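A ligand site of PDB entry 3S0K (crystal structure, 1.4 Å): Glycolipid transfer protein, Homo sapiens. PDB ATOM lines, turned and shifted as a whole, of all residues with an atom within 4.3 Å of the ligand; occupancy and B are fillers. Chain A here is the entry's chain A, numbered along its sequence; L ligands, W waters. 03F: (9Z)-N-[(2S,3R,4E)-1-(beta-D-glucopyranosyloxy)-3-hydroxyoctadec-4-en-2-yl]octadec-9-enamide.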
ATOM      1  N   LEU A  30     -17.010 -10.032 -22.948  1.00  0.00           N
ATOM      2  CA  LEU A  30     -16.505 -11.112 -22.090  1.00  0.00           C
ATOM      3  C   LEU A  30     -16.144 -12.378 -22.908  1.00  0.00           C
ATOM      4  O   LEU A  30     -15.061 -12.951 -22.725  1.00  0.00           O
ATOM      5  CB  LEU A  30     -17.488 -11.420 -20.917  1.00  0.00           C
ATOM      6  CG  LEU A  30     -17.598 -10.287 -19.887  1.00  0.00           C
ATOM      7  CD1 LEU A  30     -18.715 -10.584 -18.840  1.00  0.00           C
ATOM      8  CD2 LEU A  30     -16.303  -9.998 -19.148  1.00  0.00           C
ATOM      9  N   PHE A  33     -12.526 -13.355 -24.225  1.00  0.00           N
ATOM     10  CA  PHE A  33     -11.520 -13.863 -23.321  1.00  0.00           C
ATOM     11  C   PHE A  33     -11.292 -15.372 -23.513  1.00  0.00           C
ATOM     12  O   PHE A  33     -10.154 -15.842 -23.495  1.00  0.00           O
ATOM     13  CB  PHE A  33     -11.849 -13.613 -21.856  1.00  0.00           C
ATOM     14  CG  PHE A  33     -11.011 -14.466 -20.941  1.00  0.00           C
ATOM     15  CD1 PHE A  33      -9.715 -14.087 -20.632  1.00  0.00           C
ATOM     16  CD2 PHE A  33     -11.482 -15.675 -20.455  1.00  0.00           C
ATOM     17  CE1 PHE A  33      -8.926 -14.884 -19.815  1.00  0.00           C
ATOM     18  CE2 PHE A  33     -10.696 -16.463 -19.639  1.00  0.00           C
ATOM     19  CZ  PHE A  33      -9.424 -16.069 -19.328  1.00  0.00           C
ATOM     20  N   PHE A  34     -12.336 -16.138 -23.787  1.00  0.00           N
ATOM     21  CA  PHE A  34     -12.181 -17.574 -23.985  1.00  0.00           C
ATOM     22  C   PHE A  34     -11.234 -18.009 -25.096  1.00  0.00           C
ATOM     23  O   PHE A  34     -10.645 -19.102 -25.044  1.00  0.00           O
ATOM     24  CB  PHE A  34     -13.563 -18.201 -24.177  1.00  0.00           C
ATOM     25  CG  PHE A  34     -14.443 -18.056 -22.975  1.00  0.00           C
ATOM     26  CD1 PHE A  34     -14.127 -18.700 -21.810  1.00  0.00           C
ATOM     27  CD2 PHE A  34     -15.578 -17.296 -23.022  1.00  0.00           C
ATOM     28  CE1 PHE A  34     -14.907 -18.541 -20.690  1.00  0.00           C
ATOM     29  CE2 PHE A  34     -16.390 -17.146 -21.929  1.00  0.00           C
ATOM     30  CZ  PHE A  34     -16.051 -17.763 -20.768  1.00  0.00           C
ATOM     31  N   LEU A  37      -7.958 -19.098 -23.885  1.00  0.00           N
ATOM     32  CA  LEU A  37      -7.871 -20.356 -23.148  1.00  0.00           C
ATOM     33  C   LEU A  37      -8.016 -21.495 -24.148  1.00  0.00           C
ATOM     34  O   LEU A  37      -9.098 -21.711 -24.714  1.00  0.00           O
ATOM     35  CB  LEU A  37      -8.962 -20.470 -22.096  1.00  0.00           C
ATOM     36  CG  LEU A  37      -8.980 -19.463 -20.938  1.00  0.00           C
ATOM     37  CD1 LEU A  37     -10.077 -19.871 -19.957  1.00  0.00           C
ATOM     38  CD2 LEU A  37      -7.645 -19.351 -20.243  1.00  0.00           C
ATOM     39  N   PHE A  42     -13.507 -24.601 -23.623  1.00  0.00           N
ATOM     40  CA  PHE A  42     -13.852 -23.206 -23.753  1.00  0.00           C
ATOM     41  C   PHE A  42     -14.611 -22.861 -25.008  1.00  0.00           C
ATOM     42  O   PHE A  42     -15.300 -21.856 -25.052  1.00  0.00           O
ATOM     43  CB  PHE A  42     -12.639 -22.352 -23.444  1.00  0.00           C
ATOM     44  CG  PHE A  42     -12.159 -22.603 -22.061  1.00  0.00           C
ATOM     45  CD1 PHE A  42     -12.966 -22.246 -20.992  1.00  0.00           C
ATOM     46  CD2 PHE A  42     -11.045 -23.372 -21.809  1.00  0.00           C
ATOM     47  CE1 PHE A  42     -12.607 -22.552 -19.692  1.00  0.00           C
ATOM     48  CE2 PHE A  42     -10.661 -23.662 -20.514  1.00  0.00           C
ATOM     49  CZ  PHE A  42     -11.448 -23.269 -19.458  1.00  0.00           C
ATOM     50  N   ILE A  45     -18.281 -23.343 -24.156  1.00  0.00           N
ATOM     51  CA  ILE A  45     -18.571 -22.340 -23.087  1.00  0.00           C
ATOM     52  C   ILE A  45     -18.772 -20.996 -23.735  1.00  0.00           C
ATOM     53  O   ILE A  45     -19.728 -20.291 -23.477  1.00  0.00           O
ATOM     54  CB  ILE A  45     -17.469 -22.279 -22.059  1.00  0.00           C
ATOM     55  CG1 ILE A  45     -17.504 -23.535 -21.218  1.00  0.00           C
ATOM     56  CG2 ILE A  45     -17.581 -21.017 -21.179  1.00  0.00           C
ATOM     57  CD1 ILE A  45     -16.265 -23.720 -20.271  1.00  0.00           C
ATOM     58  N   ASP A  48     -22.023 -20.907 -25.642  1.00  0.00           N
ATOM     59  CA  ASP A  48     -23.191 -20.777 -24.758  1.00  0.00           C
ATOM     60  C   ASP A  48     -23.435 -19.358 -24.326  1.00  0.00           C
ATOM     61  O   ASP A  48     -24.547 -18.811 -24.464  1.00  0.00           O
ATOM     62  CB  ASP A  48     -23.005 -21.640 -23.514  1.00  0.00           C
ATOM     63  CG  ASP A  48     -24.183 -21.563 -22.575  1.00  0.00           C
ATOM     64  OD1 ASP A  48     -25.008 -22.480 -22.601  1.00  0.00           O
ATOM     65  OD2 ASP A  48     -24.210 -20.602 -21.806  1.00  0.00           O
ATOM     66  N   ILE A  49     -22.394 -18.709 -23.833  1.00  0.00           N
ATOM     67  CA  ILE A  49     -22.504 -17.315 -23.375  1.00  0.00           C
ATOM     68  C   ILE A  49     -22.846 -16.409 -24.533  1.00  0.00           C
ATOM     69  O   ILE A  49     -23.790 -15.645 -24.472  1.00  0.00           O
ATOM     70  CB  ILE A  49     -21.223 -16.853 -22.636  1.00  0.00           C
ATOM     71  CG1 ILE A  49     -21.010 -17.633 -21.329  1.00  0.00           C
ATOM     72  CG2 ILE A  49     -21.361 -15.368 -22.362  1.00  0.00           C
ATOM     73  CD1 ILE A  49     -19.723 -17.442 -20.684  1.00  0.00           C
ATOM     74  N   ASN A  52     -26.443 -16.797 -25.845  1.00  0.00           N
ATOM     75  CA  ASN A  52     -27.478 -16.148 -25.050  1.00  0.00           C
ATOM     76  C   ASN A  52     -27.471 -14.650 -25.227  1.00  0.00           C
ATOM     77  O   ASN A  52     -28.542 -14.059 -25.282  1.00  0.00           O
ATOM     78  CB  ASN A  52     -27.363 -16.556 -23.585  1.00  0.00           C
ATOM     79  CG  ASN A  52     -27.767 -17.994 -23.365  1.00  0.00           C
ATOM     80  OD1 ASN A  52     -28.741 -18.441 -23.969  1.00  0.00           O
ATOM     81  ND2 ASN A  52     -27.092 -18.704 -22.449  1.00  0.00           N
ATOM     82  N   LEU A  92     -35.526 -16.820 -21.266  1.00  0.00           N
ATOM     83  CA  LEU A  92     -34.756 -18.046 -21.055  1.00  0.00           C
ATOM     84  C   LEU A  92     -33.270 -17.830 -21.292  1.00  0.00           C
ATOM     85  O   LEU A  92     -32.413 -18.321 -20.533  1.00  0.00           O
ATOM     86  CB  LEU A  92     -35.272 -19.177 -21.931  1.00  0.00           C
ATOM     87  CG  LEU A  92     -34.622 -20.539 -21.708  1.00  0.00           C
ATOM     88  CD1 LEU A  92     -34.820 -21.023 -20.322  1.00  0.00           C
ATOM     89  CD2 LEU A  92     -35.254 -21.490 -22.784  1.00  0.00           C
ATOM     90  N   TRP A  96     -30.143 -18.230 -18.342  1.00  0.00           N
ATOM     91  CA  TRP A  96     -28.883 -18.949 -18.382  1.00  0.00           C
ATOM     92  C   TRP A  96     -27.653 -18.029 -18.433  1.00  0.00           C
ATOM     93  O   TRP A  96     -26.590 -18.359 -17.920  1.00  0.00           O
ATOM     94  CB  TRP A  96     -28.904 -19.936 -19.557  1.00  0.00           C
ATOM     95  CG  TRP A  96     -29.761 -21.120 -19.260  1.00  0.00           C
ATOM     96  CD1 TRP A  96     -31.032 -21.341 -19.683  1.00  0.00           C
ATOM     97  CD2 TRP A  96     -29.406 -22.240 -18.423  1.00  0.00           C
ATOM     98  NE1 TRP A  96     -31.510 -22.540 -19.157  1.00  0.00           N
ATOM     99  CE2 TRP A  96     -30.510 -23.107 -18.410  1.00  0.00           C
ATOM    100  CE3 TRP A  96     -28.261 -22.605 -17.756  1.00  0.00           C
ATOM    101  CZ2 TRP A  96     -30.464 -24.326 -17.752  1.00  0.00           C
ATOM    102  CZ3 TRP A  96     -28.235 -23.777 -17.069  1.00  0.00           C
ATOM    103  CH2 TRP A  96     -29.321 -24.639 -17.069  1.00  0.00           C
ATOM    104  N   GLY A 100     -24.058 -17.959 -16.051  1.00  0.00           N
ATOM    105  CA  GLY A 100     -22.673 -17.871 -16.521  1.00  0.00           C
ATOM    106  C   GLY A 100     -21.994 -16.614 -15.974  1.00  0.00           C
ATOM    107  O   GLY A 100     -20.837 -16.652 -15.582  1.00  0.00           O
ATOM    108  N   PHE A 103     -21.159 -17.162 -12.364  1.00  0.00           N
ATOM    109  CA  PHE A 103     -20.001 -17.996 -12.213  1.00  0.00           C
ATOM    110  C   PHE A 103     -18.724 -17.128 -12.337  1.00  0.00           C
ATOM    111  O   PHE A 103     -17.808 -17.217 -11.510  1.00  0.00           O
ATOM    112  CB  PHE A 103     -19.975 -19.101 -13.275  1.00  0.00           C
ATOM    113  CG  PHE A 103     -18.722 -19.954 -13.235  1.00  0.00           C
ATOM    114  CD1 PHE A 103     -18.736 -21.171 -12.621  1.00  0.00           C
ATOM    115  CD2 PHE A 103     -17.541 -19.508 -13.734  1.00  0.00           C
ATOM    116  CE1 PHE A 103     -17.585 -21.948 -12.574  1.00  0.00           C
ATOM    117  CE2 PHE A 103     -16.407 -20.247 -13.658  1.00  0.00           C
ATOM    118  CZ  PHE A 103     -16.425 -21.466 -13.083  1.00  0.00           C
ATOM    119  N   ILE A 104     -18.686 -16.303 -13.383  1.00  0.00           N
ATOM    120  CA  ILE A 104     -17.506 -15.464 -13.584  1.00  0.00           C
ATOM    121  C   ILE A 104     -17.289 -14.537 -12.388  1.00  0.00           C
ATOM    122  O   ILE A 104     -16.160 -14.323 -11.947  1.00  0.00           O
ATOM    123  CB  ILE A 104     -17.640 -14.683 -14.920  1.00  0.00           C
ATOM    124  CG1 ILE A 104     -17.612 -15.638 -16.133  1.00  0.00           C
ATOM    125  CG2 ILE A 104     -16.610 -13.562 -15.061  1.00  0.00           C
ATOM    126  CD1 ILE A 104     -18.056 -15.035 -17.492  1.00  0.00           C
ATOM    127  N   PHE A 107     -16.007 -16.549  -9.351  1.00  0.00           N
ATOM    128  CA  PHE A 107     -14.674 -17.080  -9.634  1.00  0.00           C
ATOM    129  C   PHE A 107     -13.655 -15.972  -9.490  1.00  0.00           C
ATOM    130  O   PHE A 107     -12.661 -16.108  -8.800  1.00  0.00           O
ATOM    131  CB  PHE A 107     -14.722 -17.616 -11.057  1.00  0.00           C
ATOM    132  CG  PHE A 107     -13.432 -18.147 -11.586  1.00  0.00           C
ATOM    133  CD1 PHE A 107     -12.767 -19.148 -10.934  1.00  0.00           C
ATOM    134  CD2 PHE A 107     -12.923 -17.654 -12.736  1.00  0.00           C
ATOM    135  CE1 PHE A 107     -11.585 -19.644 -11.423  1.00  0.00           C
ATOM    136  CE2 PHE A 107     -11.746 -18.172 -13.224  1.00  0.00           C
ATOM    137  CZ  PHE A 107     -11.114 -19.161 -12.558  1.00  0.00           C
ATOM    138  N   LEU A 108     -13.895 -14.847 -10.160  1.00  0.00           N
ATOM    139  CA  LEU A 108     -12.942 -13.740 -10.120  1.00  0.00           C
ATOM    140  C   LEU A 108     -12.851 -13.122  -8.758  1.00  0.00           C
ATOM    141  O   LEU A 108     -11.752 -12.749  -8.304  1.00  0.00           O
ATOM    142  CB  LEU A 108     -13.309 -12.659 -11.125  1.00  0.00           C
ATOM    143  CG  LEU A 108     -13.164 -13.052 -12.610  1.00  0.00           C
ATOM    144  CD1 LEU A 108     -13.666 -11.922 -13.511  1.00  0.00           C
ATOM    145  CD2 LEU A 108     -11.764 -13.444 -12.980  1.00  0.00           C
ATOM    146  N   ILE A 124      -6.196 -22.891  -9.592  1.00  0.00           N
ATOM    147  CA  ILE A 124      -7.470 -22.171  -9.430  1.00  0.00           C
ATOM    148  C   ILE A 124      -8.647 -23.125  -9.272  1.00  0.00           C
ATOM    149  O   ILE A 124      -9.800 -22.701  -9.336  1.00  0.00           O
ATOM    150  CB  ILE A 124      -7.777 -21.215 -10.615  1.00  0.00           C
ATOM    151  CG1 ILE A 124      -7.932 -22.035 -11.917  1.00  0.00           C
ATOM    152  CG2 ILE A 124      -6.725 -20.073 -10.629  1.00  0.00           C
ATOM    153  CD1 ILE A 124      -7.940 -21.230 -13.198  1.00  0.00           C
ATOM    154  N   TYR A 132     -18.615 -22.699  -9.350  1.00  0.00           N
ATOM    155  CA  TYR A 132     -19.503 -23.734  -9.927  1.00  0.00           C
ATOM    156  C   TYR A 132     -20.616 -24.084  -8.957  1.00  0.00           C
ATOM    157  O   TYR A 132     -21.786 -24.152  -9.341  1.00  0.00           O
ATOM    158  CB  TYR A 132     -18.689 -24.977 -10.275  1.00  0.00           C
ATOM    159  CG  TYR A 132     -19.466 -25.978 -11.048  1.00  0.00           C
ATOM    160  CD1 TYR A 132     -19.875 -25.716 -12.349  1.00  0.00           C
ATOM    161  CD2 TYR A 132     -19.755 -27.219 -10.521  1.00  0.00           C
ATOM    162  CE1 TYR A 132     -20.611 -26.611 -13.073  1.00  0.00           C
ATOM    163  CE2 TYR A 132     -20.485 -28.144 -11.255  1.00  0.00           C
ATOM    164  CZ  TYR A 132     -20.920 -27.847 -12.524  1.00  0.00           C
ATOM    165  OH  TYR A 132     -21.597 -28.770 -13.325  1.00  0.00           O
ATOM    166  N   LEU A 136     -23.854 -22.782 -10.944  1.00  0.00           N
ATOM    167  CA  LEU A 136     -24.234 -23.666 -12.033  1.00  0.00           C
ATOM    168  C   LEU A 136     -24.614 -25.079 -11.586  1.00  0.00           C
ATOM    169  O   LEU A 136     -25.449 -25.696 -12.186  1.00  0.00           O
ATOM    170  CB  LEU A 136     -23.078 -23.802 -13.017  1.00  0.00           C
ATOM    171  CG  LEU A 136     -22.789 -22.549 -13.837  1.00  0.00           C
ATOM    172  CD1 LEU A 136     -21.514 -22.749 -14.608  1.00  0.00           C
ATOM    173  CD2 LEU A 136     -23.960 -22.146 -14.705  1.00  0.00           C
ATOM    174  N   HIS A 140     -27.155 -28.650 -13.402  1.00  0.00           N
ATOM    175  CA  HIS A 140     -26.432 -29.541 -14.276  1.00  0.00           C
ATOM    176  C   HIS A 140     -26.611 -30.996 -13.890  1.00  0.00           C
ATOM    177  O   HIS A 140     -26.316 -31.377 -12.750  1.00  0.00           O
ATOM    178  CB  HIS A 140     -24.941 -29.254 -14.256  1.00  0.00           C
ATOM    179  CG  HIS A 140     -24.559 -28.036 -15.004  1.00  0.00           C
ATOM    180  ND1 HIS A 140     -23.273 -27.535 -15.004  1.00  0.00           N
ATOM    181  CD2 HIS A 140     -25.302 -27.194 -15.779  1.00  0.00           C
ATOM    182  CE1 HIS A 140     -23.246 -26.433 -15.744  1.00  0.00           C
ATOM    183  NE2 HIS A 140     -24.466 -26.196 -16.212  1.00  0.00           N
ATOM    184  N   VAL A 144     -23.288 -33.062 -17.867  1.00  0.00           N
ATOM    185  CA  VAL A 144     -22.684 -31.709 -17.923  1.00  0.00           C
ATOM    186  C   VAL A 144     -21.696 -31.521 -16.789  1.00  0.00           C
ATOM    187  O   VAL A 144     -20.683 -30.849 -16.930  1.00  0.00           O
ATOM    188  CB  VAL A 144     -23.765 -30.653 -17.915  1.00  0.00           C
ATOM    189  CG1 VAL A 144     -23.153 -29.236 -17.946  1.00  0.00           C
ATOM    190  CG2 VAL A 144     -24.634 -30.804 -19.176  1.00  0.00           C
ATOM    191  N   PHE A 148     -17.502 -29.998 -16.416  1.00  0.00           N
ATOM    192  CA  PHE A 148     -16.856 -29.169 -15.404  1.00  0.00           C
ATOM    193  C   PHE A 148     -15.657 -29.894 -14.812  1.00  0.00           C
ATOM    194  O   PHE A 148     -14.575 -29.296 -14.582  1.00  0.00           O
ATOM    195  CB  PHE A 148     -17.823 -28.782 -14.298  1.00  0.00           C
ATOM    196  CG  PHE A 148     -17.146 -28.086 -13.160  1.00  0.00           C
ATOM    197  CD1 PHE A 148     -16.687 -26.798 -13.347  1.00  0.00           C
ATOM    198  CD2 PHE A 148     -16.839 -28.731 -11.984  1.00  0.00           C
ATOM    199  CE1 PHE A 148     -16.004 -26.157 -12.347  1.00  0.00           C
ATOM    200  CE2 PHE A 148     -16.189 -28.037 -10.975  1.00  0.00           C
ATOM    201  CZ  PHE A 148     -15.779 -26.772 -11.174  1.00  0.00           C
ATOM    202  N   ALA A 151     -12.795 -29.815 -17.208  1.00  0.00           N
ATOM    203  CA  ALA A 151     -12.253 -28.436 -17.208  1.00  0.00           C
ATOM    204  C   ALA A 151     -11.389 -28.133 -15.996  1.00  0.00           C
ATOM    205  O   ALA A 151     -10.352 -27.465 -16.119  1.00  0.00           O
ATOM    206  CB  ALA A 151     -13.345 -27.416 -17.277  1.00  0.00           C
ATOM    207  N   PHE A 161      -3.324 -18.005 -15.909  1.00  0.00           N
ATOM    208  CA  PHE A 161      -4.656 -17.501 -16.139  1.00  0.00           C
ATOM    209  C   PHE A 161      -4.652 -16.004 -16.034  1.00  0.00           C
ATOM    210  O   PHE A 161      -5.249 -15.301 -16.847  1.00  0.00           O
ATOM    211  CB  PHE A 161      -5.601 -18.094 -15.094  1.00  0.00           C
ATOM    212  CG  PHE A 161      -6.956 -17.463 -15.087  1.00  0.00           C
ATOM    213  CD1 PHE A 161      -7.827 -17.659 -16.144  1.00  0.00           C
ATOM    214  CD2 PHE A 161      -7.361 -16.667 -14.042  1.00  0.00           C
ATOM    215  CE1 PHE A 161      -9.063 -17.090 -16.147  1.00  0.00           C
ATOM    216  CE2 PHE A 161      -8.589 -16.055 -14.059  1.00  0.00           C
ATOM    217  CZ  PHE A 161      -9.440 -16.288 -15.116  1.00  0.00           C
ATOM    218  N   LEU A 165      -5.776 -12.958 -18.812  1.00  0.00           N
ATOM    219  CA  LEU A 165      -6.703 -11.841 -18.544  1.00  0.00           C
ATOM    220  C   LEU A 165      -6.123 -10.475 -18.911  1.00  0.00           C
ATOM    221  O   LEU A 165      -6.891  -9.542 -19.224  1.00  0.00           O
ATOM    222  CB  LEU A 165      -7.136 -11.796 -17.084  1.00  0.00           C
ATOM    223  CG  LEU A 165      -8.343 -12.636 -16.698  1.00  0.00           C
ATOM    224  CD1 LEU A 165      -8.592 -12.458 -15.238  1.00  0.00           C
ATOM    225  CD2 LEU A 165      -9.567 -12.215 -17.531  1.00  0.00           C
ATOM    226  N   PHE A 183     -13.778  -3.673 -11.908  1.00  0.00           N
ATOM    227  CA  PHE A 183     -14.779  -4.241 -12.805  1.00  0.00           C
ATOM    228  C   PHE A 183     -15.902  -4.932 -12.034  1.00  0.00           C
ATOM    229  O   PHE A 183     -17.067  -4.820 -12.340  1.00  0.00           O
ATOM    230  CB  PHE A 183     -14.119  -5.184 -13.789  1.00  0.00           C
ATOM    231  CG  PHE A 183     -15.070  -6.104 -14.457  1.00  0.00           C
ATOM    232  CD1 PHE A 183     -15.828  -5.710 -15.524  1.00  0.00           C
ATOM    233  CD2 PHE A 183     -15.175  -7.390 -13.959  1.00  0.00           C
ATOM    234  CE1 PHE A 183     -16.740  -6.689 -16.092  1.00  0.00           C
ATOM    235  CE2 PHE A 183     -16.009  -8.284 -14.481  1.00  0.00           C
ATOM    236  CZ  PHE A 183     -16.786  -7.937 -15.552  1.00  0.00           C
ATOM    237  N   TYR A 207     -34.803 -26.608 -13.520  1.00  0.00           N
ATOM    238  CA  TYR A 207     -34.530 -27.823 -14.271  1.00  0.00           C
ATOM    239  C   TYR A 207     -33.037 -28.019 -14.493  1.00  0.00           C
ATOM    240  O   TYR A 207     -32.266 -27.080 -14.592  1.00  0.00           O
ATOM    241  CB  TYR A 207     -35.338 -27.865 -15.566  1.00  0.00           C
ATOM    242  CG  TYR A 207     -34.891 -26.932 -16.697  1.00  0.00           C
ATOM    243  CD1 TYR A 207     -33.995 -27.365 -17.641  1.00  0.00           C
ATOM    244  CD2 TYR A 207     -35.361 -25.643 -16.806  1.00  0.00           C
ATOM    245  CE1 TYR A 207     -33.603 -26.579 -18.695  1.00  0.00           C
ATOM    246  CE2 TYR A 207     -34.928 -24.804 -17.838  1.00  0.00           C
ATOM    247  CZ  TYR A 207     -34.094 -25.284 -18.792  1.00  0.00           C
ATOM    248  OH  TYR A 207     -33.637 -24.480 -19.794  1.00  0.00           O
ATOM    249  N   VAL A 209     -29.990 -29.717 -16.988  1.00  0.00           N
ATOM    250  CA  VAL A 209     -29.655 -30.013 -18.350  1.00  0.00           C
ATOM    251  C   VAL A 209     -28.659 -31.166 -18.402  1.00  0.00           C
ATOM    252  O   VAL A 209     -28.533 -31.728 -19.510  1.00  0.00           O
ATOM    253  CB  VAL A 209     -29.087 -28.797 -19.109  1.00  0.00           C
ATOM    254  CG1 VAL A 209     -30.176 -27.767 -19.210  1.00  0.00           C
ATOM    255  CG2 VAL A 209     -27.874 -28.190 -18.422  1.00  0.00           C
ATOM    256  OXT VAL A 209     -27.993 -31.483 -17.400  1.00  0.00           O
HETATM  257  C1  03F L   1     -27.515 -25.016 -20.624  1.00  0.00           C
HETATM  258  C2  03F L   1     -26.086 -25.134 -20.147  1.00  0.00           C
HETATM  259  N2  03F L   1     -25.549 -23.762 -19.975  1.00  0.00           N
HETATM  260  C3  03F L   1     -25.217 -25.875 -21.129  1.00  0.00           C
HETATM  261  O3  03F L   1     -25.793 -27.203 -21.199  1.00  0.00           O
HETATM  262  C4  03F L   1     -23.793 -26.035 -20.619  1.00  0.00           C
HETATM  263  C5  03F L   1     -22.774 -25.501 -21.225  1.00  0.00           C
HETATM  264  C6  03F L   1     -21.366 -25.684 -20.651  1.00  0.00           C
HETATM  265  C7  03F L   1     -21.233 -25.899 -19.140  1.00  0.00           C
HETATM  266  C8  03F L   1     -19.790 -25.630 -18.659  1.00  0.00           C
HETATM  267  C9  03F L   1     -19.638 -26.007 -17.170  1.00  0.00           C
HETATM  268  C10 03F L   1     -18.495 -25.333 -16.408  1.00  0.00           C
HETATM  269  C11 03F L   1     -17.295 -24.924 -17.239  1.00  0.00           C
HETATM  270  C12 03F L   1     -15.874 -25.041 -16.671  1.00  0.00           C
HETATM  271  C13 03F L   1     -15.400 -23.723 -16.054  1.00  0.00           C
HETATM  272  C14 03F L   1     -13.955 -23.816 -15.571  1.00  0.00           C
HETATM  273  C15 03F L   1     -13.267 -22.484 -15.665  1.00  0.00           C
HETATM  274  C16 03F L   1     -11.780 -22.550 -15.360  1.00  0.00           C
HETATM  275  C17 03F L   1     -11.157 -21.155 -15.512  1.00  0.00           C
HETATM  276  C18 03F L   1     -10.614 -20.837 -16.907  1.00  0.00           C
HETATM  277  C1A 03F L   1     -28.749 -23.517 -21.978  1.00  0.00           C
HETATM  278  O1A 03F L   1     -27.599 -24.247 -21.763  1.00  0.00           O
HETATM  279  C2A 03F L   1     -28.489 -22.519 -23.051  1.00  0.00           C
HETATM  280  O2A 03F L   1     -27.518 -21.557 -22.540  1.00  0.00           O
HETATM  281  C3A 03F L   1     -29.752 -21.782 -23.395  1.00  0.00           C
HETATM  282  O3A 03F L   1     -29.544 -20.934 -24.533  1.00  0.00           O
HETATM  283  C4A 03F L   1     -30.909 -22.766 -23.702  1.00  0.00           C
HETATM  284  O4A 03F L   1     -32.090 -22.022 -23.885  1.00  0.00           O
HETATM  285  O5A 03F L   1     -32.247 -25.661 -21.727  1.00  0.00           O
HETATM  286  C5M 03F L   1     -30.978 -23.783 -22.560  1.00  0.00           C
HETATM  287  C6A 03F L   1     -32.104 -24.778 -22.809  1.00  0.00           C
HETATM  288  O6A 03F L   1     -29.742 -24.460 -22.378  1.00  0.00           O
HETATM  289  CAA 03F L   1     -24.968 -23.368 -18.746  1.00  0.00           C
HETATM  290  OAA 03F L   1     -24.932 -24.019 -17.730  1.00  0.00           O
HETATM  291  CAB 03F L   1     -24.300 -22.014 -18.638  1.00  0.00           C
HETATM  292  CAC 03F L   1     -22.778 -22.228 -18.671  1.00  0.00           C
HETATM  293  CAD 03F L   1     -21.893 -20.984 -18.329  1.00  0.00           C
HETATM  294  CAE 03F L   1     -20.401 -21.295 -18.240  1.00  0.00           C
HETATM  295  CAF 03F L   1     -19.502 -20.190 -17.831  1.00  0.00           C
HETATM  296  CAG 03F L   1     -18.066 -20.582 -17.539  1.00  0.00           C
HETATM  297  CAH 03F L   1     -17.091 -19.407 -17.516  1.00  0.00           C
HETATM  298  CAI 03F L   1     -15.673 -19.975 -17.392  1.00  0.00           C
HETATM  299  CAJ 03F L   1     -14.544 -19.301 -17.133  1.00  0.00           C
HETATM  300  CAK 03F L   1     -14.559 -17.840 -17.003  1.00  0.00           C
HETATM  301  CAL 03F L   1     -13.414 -16.837 -16.989  1.00  0.00           C
HETATM  302  CAM 03F L   1     -13.830 -15.543 -17.699  1.00  0.00           C
HETATM  303  CAN 03F L   1     -12.960 -14.354 -17.342  1.00  0.00           C
HETATM  304  CAO 03F L   1     -13.421 -13.026 -17.928  1.00  0.00           C
HETATM  305  CAP 03F L   1     -13.215 -11.912 -16.914  1.00  0.00           C
HETATM  306  CAQ 03F L   1     -13.418 -10.514 -17.464  1.00  0.00           C
HETATM  307  CAR 03F L   1     -12.840  -9.468 -16.529  1.00  0.00           C
HETATM  308  O   HOH W   1     -30.813 -27.642 -22.483  1.00  0.00           O
HETATM  309  O   HOH W   2     -32.143 -19.468 -24.849  1.00  0.00           O
HETATM  310  O   HOH W   3     -29.168 -22.341 -26.928  1.00  0.00           O
HETATM  311  O   HOH W   4     -30.367 -18.439 -26.383  1.00  0.00           O
HETATM  312  O   HOH W   5     -24.122 -28.942 -22.513  1.00  0.00           O
HETATM  313  O   HOH W   6     -26.552 -20.453 -25.548  1.00  0.00           O
HETATM  314  O   HOH W   7     -28.010 -27.831 -22.797  1.00  0.00           O
HETATM  315  O   HOH W   8     -33.600 -23.243 -25.668  1.00  0.00           O
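ND1 of His 140 sits at hydrogen-bond distance from OH of Tyr 132 (2.7 Å).
O of Asp 48 is in hydrogen-bond range of ND2 of Asn 52, at 3.2 Å.
The side-chain hydroxyl (OH) of Tyr 207 lies within hydrogen-bond range of the indole nitrogen (NE1) of Trp 96 (2.9 Å).
An oxygen (O5A) of the ligand lies within hydrogen-bond range of the side-chain hydroxyl (OH) of Tyr 207, at 2.7 Å.
OD1 of Asp 48 is in hydrogen-bond range of O2A of the ligand, 2.7 Å away.
The side-chain amide oxygen of Asn 52 sits at hydrogen-bond distance from an oxygen (O3A) of the ligand (2.7 Å).
NE2 of His 140 lies within hydrogen-bond range of OAA of the ligand (2.7 Å).
Leu 30 touches the ligand (CD2 to CAQ, 3.4 Å).
Phe 33 touches the ligand (CD2 to CAM, 3.6 Å).
CE1 of Phe 34 touches CAJ of the ligand, at 3.7 Å.
CD1 of Leu 37 touches C18 of the ligand, 3.2 Å away.
Phe 42 touches the ligand (CZ to C18, 3.6 Å).
CD1 of Ile 45 touches C11 of the ligand, at 3.4 Å.
Ile 49 touches the ligand.
Leu 92 touches the ligand.
Trp 96 touches the ligand (CZ3 to OAA, 3.4 Å).
Gly 100 touches the ligand.
Phe 103 touches the ligand.
Ile 104 touches the ligand (CG1 to CAK, 3.9 Å).
Phe 107 touches the ligand (CZ to C17, 3.6 Å).
CD1 of Leu 108 touches CAP of the ligand, 3.4 Å away.
CD1 of Ile 124 touches C17 of the ligand, at 3.96 Å.
Leu 136 touches the ligand.
Phe 148 touches the ligand.
Ala 151 touches the ligand.
Leu 165 touches the ligand.
CE2 of Phe 183 touches CAR of the ligand (3.95 Å).
Val 209 touches the ligand.
Hydrophobic or aromatic side chains within 4 Å of the ligand: Leu 30, Phe 33, Phe 34, Leu 37, Phe 42, Ile 45, Ile 49, Leu 92, Trp 96, Phe 103, Ile 104, Phe 107, Leu 108, Ile 124, Leu 136, His 140, Phe 148, Ala 151, Leu 165, Phe 183, Tyr 207 and Val 209.
25 residues have an atom within 4 Å of the ligand: Leu 30, Phe 33, Phe 34, Leu 37, Phe 42, Ile 45, Asp 48, Ile 49, Asn 52, Leu 92, Trp 96, Gly 100, Phe 103, Ile 104, Phe 107, Leu 108, Ile 124, Leu 136, His 140, Phe 148, Ala 151, Leu 165, Phe 183, Tyr 207 and Val 209.
The nearest printed residue that does not touch the ligand is Val 144 (4.03 Å).
Water W6 lies within hydrogen-bond range of O of Asp 48 (2.8 Å), O3A of the ligand (3.2 Å) and OD1 of Asn 52 (3.4 Å).
Water W4 lies within hydrogen-bond range of the side-chain amide oxygen of Asn 52 (2.9 Å) and an oxygen (O3A) of the ligand (3.2 Å).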
